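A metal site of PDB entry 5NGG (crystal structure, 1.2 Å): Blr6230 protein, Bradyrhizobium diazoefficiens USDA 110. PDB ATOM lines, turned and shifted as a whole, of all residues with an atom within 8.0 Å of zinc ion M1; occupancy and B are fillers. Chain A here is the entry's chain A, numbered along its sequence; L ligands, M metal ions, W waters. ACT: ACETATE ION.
The backbone carbonyl oxygen of Gly 54 sits at hydrogen-bond distance from a ring nitrogen (ND1) of His 242, 2.8 Å away. A ring nitrogen (ND1) of His 101 lies within hydrogen-bond range of the backbone carbonyl oxygen of Cys 201, at 2.7 Å.
Residues that only touch zinc ion M1: His 101 (3.99 Å). The nearest printed residue that does not touch zinc ion M1 is Trp 34 (4.4 Å).
Zinc ion M1 is bound by a ring nitrogen (NE2) of His 106 (2.0 Å), water W1 (2.1 Å), a ring nitrogen (NE2) of His 242 (2.1 Å), the side-chain carboxylate of Asp 105 (2.1 Å) and an oxygen (OXT) of the ligand (2.2 Å).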
ATOM      1  N   PHE A  26      10.901 -18.510  33.059  1.00  0.00           N
ATOM      2  CA  PHE A  26       9.532 -18.687  32.559  1.00  0.00           C
ATOM      3  C   PHE A  26       8.778 -17.353  32.605  1.00  0.00           C
ATOM      4  O   PHE A  26       8.143 -16.971  31.613  1.00  0.00           O
ATOM      5  CB  PHE A  26       8.798 -19.747  33.378  1.00  0.00           C
ATOM      6  CG  PHE A  26       7.355 -19.912  33.019  1.00  0.00           C
ATOM      7  CD1 PHE A  26       6.368 -19.159  33.663  1.00  0.00           C
ATOM      8  CD2 PHE A  26       6.959 -20.834  32.076  1.00  0.00           C
ATOM      9  CE1 PHE A  26       5.028 -19.314  33.347  1.00  0.00           C
ATOM     10  CE2 PHE A  26       5.619 -20.999  31.763  1.00  0.00           C
ATOM     11  CZ  PHE A  26       4.655 -20.243  32.390  1.00  0.00           C
ATOM     12  N   TRP A  34       5.524 -13.427  25.150  1.00  0.00           N
ATOM     13  CA  TRP A  34       4.196 -13.833  25.443  1.00  0.00           C
ATOM     14  C   TRP A  34       3.200 -12.696  25.495  1.00  0.00           C
ATOM     15  O   TRP A  34       2.033 -12.940  25.285  1.00  0.00           O
ATOM     16  CB  TRP A  34       4.171 -14.640  26.721  1.00  0.00           C
ATOM     17  CG  TRP A  34       4.761 -16.038  26.592  1.00  0.00           C
ATOM     18  CD1 TRP A  34       5.549 -16.508  25.578  1.00  0.00           C
ATOM     19  CD2 TRP A  34       4.655 -17.119  27.537  1.00  0.00           C
ATOM     20  NE1 TRP A  34       5.907 -17.814  25.820  1.00  0.00           N
ATOM     21  CE2 TRP A  34       5.367 -18.206  27.017  1.00  0.00           C
ATOM     22  CE3 TRP A  34       4.009 -17.259  28.768  1.00  0.00           C
ATOM     23  CZ2 TRP A  34       5.456 -19.435  27.669  1.00  0.00           C
ATOM     24  CZ3 TRP A  34       4.105 -18.475  29.428  1.00  0.00           C
ATOM     25  CH2 TRP A  34       4.835 -19.544  28.873  1.00  0.00           C
ATOM     26  N   GLY A  54       3.529 -15.029  21.313  1.00  0.00           N
ATOM     27  CA  GLY A  54       4.002 -16.205  22.026  1.00  0.00           C
ATOM     28  C   GLY A  54       2.948 -17.070  22.653  1.00  0.00           C
ATOM     29  O   GLY A  54       3.319 -18.144  23.129  1.00  0.00           O
ATOM     30  N   ILE A  55       1.674 -16.658  22.656  1.00  0.00           N
ATOM     31  CA  ILE A  55       0.578 -17.444  23.233  1.00  0.00           C
ATOM     32  C   ILE A  55      -0.560 -17.443  22.197  1.00  0.00           C
ATOM     33  O   ILE A  55      -1.002 -16.373  21.760  1.00  0.00           O
ATOM     34  CB  ILE A  55       0.065 -16.867  24.558  1.00  0.00           C
ATOM     35  CG1 ILE A  55       1.154 -16.975  25.644  1.00  0.00           C
ATOM     36  CG2 ILE A  55      -1.206 -17.606  25.000  1.00  0.00           C
ATOM     37  CD1 ILE A  55       0.870 -16.174  26.886  1.00  0.00           C
ATOM     38  N   ALA A  56      -1.005 -18.621  21.807  1.00  0.00           N
ATOM     39  CA  ALA A  56      -2.059 -18.771  20.781  1.00  0.00           C
ATOM     40  C   ALA A  56      -3.428 -18.772  21.428  1.00  0.00           C
ATOM     41  O   ALA A  56      -3.687 -19.524  22.377  1.00  0.00           O
ATOM     42  CB  ALA A  56      -1.822 -20.064  20.027  1.00  0.00           C
ATOM     43  N   MET A  73      -1.936 -14.387  29.216  1.00  0.00           N
ATOM     44  CA  MET A  73      -1.566 -14.010  30.563  1.00  0.00           C
ATOM     45  C   MET A  73      -2.632 -13.095  31.172  1.00  0.00           C
ATOM     46  O   MET A  73      -3.320 -12.391  30.419  1.00  0.00           O
ATOM     47  CB  MET A  73      -0.216 -13.309  30.592  1.00  0.00           C
ATOM     48  CG  MET A  73       0.977 -14.201  30.278  1.00  0.00           C
ATOM     49  SD  MET A  73       1.357 -15.382  31.582  1.00  0.00           S
ATOM     50  CE  MET A  73       2.152 -14.315  32.785  1.00  0.00           C
ATOM     51  N   THR A 100      -7.636 -25.582  26.800  1.00  0.00           N
ATOM     52  CA  THR A 100      -6.721 -26.707  26.561  1.00  0.00           C
ATOM     53  C   THR A 100      -6.153 -27.194  27.904  1.00  0.00           C
ATOM     54  O   THR A 100      -6.243 -28.362  28.251  1.00  0.00           O
ATOM     55  CB  THR A 100      -5.546 -26.326  25.639  1.00  0.00           C
ATOM     56  OG1 THR A 100      -4.927 -25.125  26.117  1.00  0.00           O
ATOM     57  CG2 THR A 100      -6.019 -26.210  24.194  1.00  0.00           C
ATOM     58  N   HIS A 101      -5.564 -26.289  28.681  1.00  0.00           N
ATOM     59  CA  HIS A 101      -5.033 -26.698  29.998  1.00  0.00           C
ATOM     60  C   HIS A 101      -4.917 -25.500  30.925  1.00  0.00           C
ATOM     61  O   HIS A 101      -4.786 -24.356  30.488  1.00  0.00           O
ATOM     62  CB  HIS A 101      -3.715 -27.461  29.884  1.00  0.00           C
ATOM     63  CG  HIS A 101      -2.534 -26.585  29.600  1.00  0.00           C
ATOM     64  ND1 HIS A 101      -2.043 -26.367  28.324  1.00  0.00           N
ATOM     65  CD2 HIS A 101      -1.707 -25.937  30.441  1.00  0.00           C
ATOM     66  CE1 HIS A 101      -0.984 -25.578  28.404  1.00  0.00           C
ATOM     67  NE2 HIS A 101      -0.768 -25.277  29.666  1.00  0.00           N
ATOM     68  N   HIS A 103      -3.123 -23.504  33.038  1.00  0.00           N
ATOM     69  CA  HIS A 103      -1.997 -22.681  33.492  1.00  0.00           C
ATOM     70  C   HIS A 103      -2.265 -21.234  33.154  1.00  0.00           C
ATOM     71  O   HIS A 103      -2.975 -20.935  32.185  1.00  0.00           O
ATOM     72  CB  HIS A 103      -0.684 -23.108  32.827  1.00  0.00           C
ATOM     73  CG  HIS A 103      -0.180 -24.434  33.242  1.00  0.00           C
ATOM     74  ND1 HIS A 103       0.692 -25.152  32.470  1.00  0.00           N
ATOM     75  CD2 HIS A 103      -0.396 -25.171  34.360  1.00  0.00           C
ATOM     76  CE1 HIS A 103       1.011 -26.267  33.091  1.00  0.00           C
ATOM     77  NE2 HIS A 103       0.359 -26.308  34.241  1.00  0.00           N
ATOM     78  N   LEU A 104      -1.703 -20.338  33.960  1.00  0.00           N
ATOM     79  CA  LEU A 104      -2.019 -18.895  33.874  1.00  0.00           C
ATOM     80  C   LEU A 104      -1.796 -18.257  32.510  1.00  0.00           C
ATOM     81  O   LEU A 104      -2.451 -17.276  32.209  1.00  0.00           O
ATOM     82  CB  LEU A 104      -1.274 -18.093  34.923  1.00  0.00           C
ATOM     83  CG  LEU A 104       0.170 -17.670  34.662  1.00  0.00           C
ATOM     84  CD1 LEU A 104       0.593 -16.576  35.647  1.00  0.00           C
ATOM     85  CD2 LEU A 104       1.105 -18.852  34.745  1.00  0.00           C
ATOM     86  N   ASP A 105      -0.870 -18.788  31.704  1.00  0.00           N
ATOM     87  CA  ASP A 105      -0.625 -18.241  30.390  1.00  0.00           C
ATOM     88  C   ASP A 105      -1.721 -18.570  29.388  1.00  0.00           C
ATOM     89  O   ASP A 105      -1.730 -18.009  28.281  1.00  0.00           O
ATOM     90  CB  ASP A 105       0.768 -18.625  29.859  1.00  0.00           C
ATOM     91  CG  ASP A 105       1.096 -20.112  29.855  1.00  0.00           C
ATOM     92  OD1 ASP A 105       0.712 -20.835  30.807  1.00  0.00           O
ATOM     93  OD2 ASP A 105       1.766 -20.509  28.850  1.00  0.00           O
ATOM     94  N   HIS A 106      -2.670 -19.432  29.776  1.00  0.00           N
ATOM     95  CA  HIS A 106      -3.827 -19.770  28.949  1.00  0.00           C
ATOM     96  C   HIS A 106      -5.166 -19.438  29.610  1.00  0.00           C
ATOM     97  O   HIS A 106      -6.191 -19.402  28.927  1.00  0.00           O
ATOM     98  CB  HIS A 106      -3.790 -21.243  28.554  1.00  0.00           C
ATOM     99  CG  HIS A 106      -2.451 -21.635  27.991  1.00  0.00           C
ATOM    100  ND1 HIS A 106      -1.993 -21.156  26.785  1.00  0.00           N
ATOM    101  CD2 HIS A 106      -1.419 -22.305  28.539  1.00  0.00           C
ATOM    102  CE1 HIS A 106      -0.743 -21.542  26.614  1.00  0.00           C
ATOM    103  NE2 HIS A 106      -0.368 -22.263  27.660  1.00  0.00           N
ATOM    104  N   HIS A 177       1.112 -32.520  30.670  1.00  0.00           N
ATOM    105  CA  HIS A 177       1.494 -31.139  30.905  1.00  0.00           C
ATOM    106  C   HIS A 177       0.616 -30.527  32.031  1.00  0.00           C
ATOM    107  O   HIS A 177       1.084 -29.682  32.802  1.00  0.00           O
ATOM    108  CB  HIS A 177       1.425 -30.350  29.590  1.00  0.00           C
ATOM    109  CG  HIS A 177       1.829 -28.921  29.724  1.00  0.00           C
ATOM    110  ND1 HIS A 177       3.129 -28.485  29.686  1.00  0.00           N
ATOM    111  CD2 HIS A 177       1.072 -27.831  29.948  1.00  0.00           C
ATOM    112  CE1 HIS A 177       3.150 -27.164  29.846  1.00  0.00           C
ATOM    113  NE2 HIS A 177       1.917 -26.752  30.033  1.00  0.00           N
ATOM    114  N   CYS A 201      -3.163 -29.804  23.333  1.00  0.00           N
ATOM    115  CA  CYS A 201      -3.159 -29.070  24.581  1.00  0.00           C
ATOM    116  C   CYS A 201      -1.836 -28.623  25.113  1.00  0.00           C
ATOM    117  O   CYS A 201      -1.847 -27.780  26.010  1.00  0.00           O
ATOM    118  CB  CYS A 201      -3.899 -29.875  25.665  1.00  0.00           C
ATOM    119  SG  CYS A 201      -2.983 -31.245  26.348  1.00  0.00           S
ATOM    120  N   SER A 202      -0.755 -29.209  24.626  1.00  0.00           N
ATOM    121  CA  SER A 202       0.663 -29.066  25.096  1.00  0.00           C
ATOM    122  C   SER A 202       1.161 -30.391  25.630  1.00  0.00           C
ATOM    123  O   SER A 202       0.471 -31.014  26.429  1.00  0.00           O
ATOM    124  CB  SER A 202       0.939 -28.050  26.195  1.00  0.00           C
ATOM    125  OG  SER A 202       2.317 -28.177  26.559  1.00  0.00           O
ATOM    126  N   THR A 204       4.800 -30.323  26.624  1.00  0.00           N
ATOM    127  CA  THR A 204       6.118 -29.938  27.101  1.00  0.00           C
ATOM    128  C   THR A 204       6.268 -30.264  28.591  1.00  0.00           C
ATOM    129  O   THR A 204       5.260 -30.296  29.325  1.00  0.00           O
ATOM    130  CB  THR A 204       6.370 -28.439  26.900  1.00  0.00           C
ATOM    131  OG1 THR A 204       5.414 -27.744  27.682  1.00  0.00           O
ATOM    132  CG2 THR A 204       6.286 -28.026  25.426  1.00  0.00           C
ATOM    133  N   ALA A 206       8.271 -28.268  30.644  1.00  0.00           N
ATOM    134  CA  ALA A 206       8.164 -26.895  31.136  1.00  0.00           C
ATOM    135  C   ALA A 206       8.497 -26.875  32.640  1.00  0.00           C
ATOM    136  O   ALA A 206       9.598 -27.330  32.995  1.00  0.00           O
ATOM    137  CB  ALA A 206       6.793 -26.318  30.782  1.00  0.00           C
ATOM    138  N   PRO A 241      -1.459 -24.289  21.977  1.00  0.00           N
ATOM    139  CA  PRO A 241      -1.647 -23.091  22.799  1.00  0.00           C
ATOM    140  C   PRO A 241      -0.469 -22.120  22.784  1.00  0.00           C
ATOM    141  O   PRO A 241      -0.578 -21.035  23.361  1.00  0.00           O
ATOM    142  CB  PRO A 241      -1.938 -23.644  24.181  1.00  0.00           C
ATOM    143  CG  PRO A 241      -1.275 -24.956  24.213  1.00  0.00           C
ATOM    144  CD  PRO A 241      -1.175 -25.477  22.802  1.00  0.00           C
ATOM    145  N   HIS A 242       0.614 -22.483  22.084  1.00  0.00           N
ATOM    146  CA  HIS A 242       1.725 -21.588  21.787  1.00  0.00           C
ATOM    147  C   HIS A 242       2.008 -21.753  20.298  1.00  0.00           C
ATOM    148  O   HIS A 242       1.969 -22.880  19.789  1.00  0.00           O
ATOM    149  CB  HIS A 242       2.969 -21.931  22.626  1.00  0.00           C
ATOM    150  CG  HIS A 242       2.782 -21.695  24.089  1.00  0.00           C
ATOM    151  ND1 HIS A 242       2.862 -20.448  24.673  1.00  0.00           N
ATOM    152  CD2 HIS A 242       2.515 -22.556  25.089  1.00  0.00           C
ATOM    153  CE1 HIS A 242       2.659 -20.574  25.983  1.00  0.00           C
ATOM    154  NE2 HIS A 242       2.435 -21.836  26.256  1.00  0.00           N
HETATM  155  C   ACT L   1       3.305 -24.860  27.421  1.00  0.00           C
HETATM  156  O   ACT L   1       3.663 -25.880  26.825  1.00  0.00           O
HETATM  157  OXT ACT L   1       2.082 -24.537  27.480  1.00  0.00           O
HETATM  158  CH3 ACT L   1       4.370 -24.023  28.053  1.00  0.00           C
HETATM  159 ZN    ZN M   1       1.621 -22.493  28.098  1.00  0.00          ZN
HETATM  160 ZN    ZN M   2       1.105 -24.898  30.452  1.00  0.00          ZN
HETATM  161  O   HOH W   1       1.811 -23.236  30.004  1.00  0.00           O
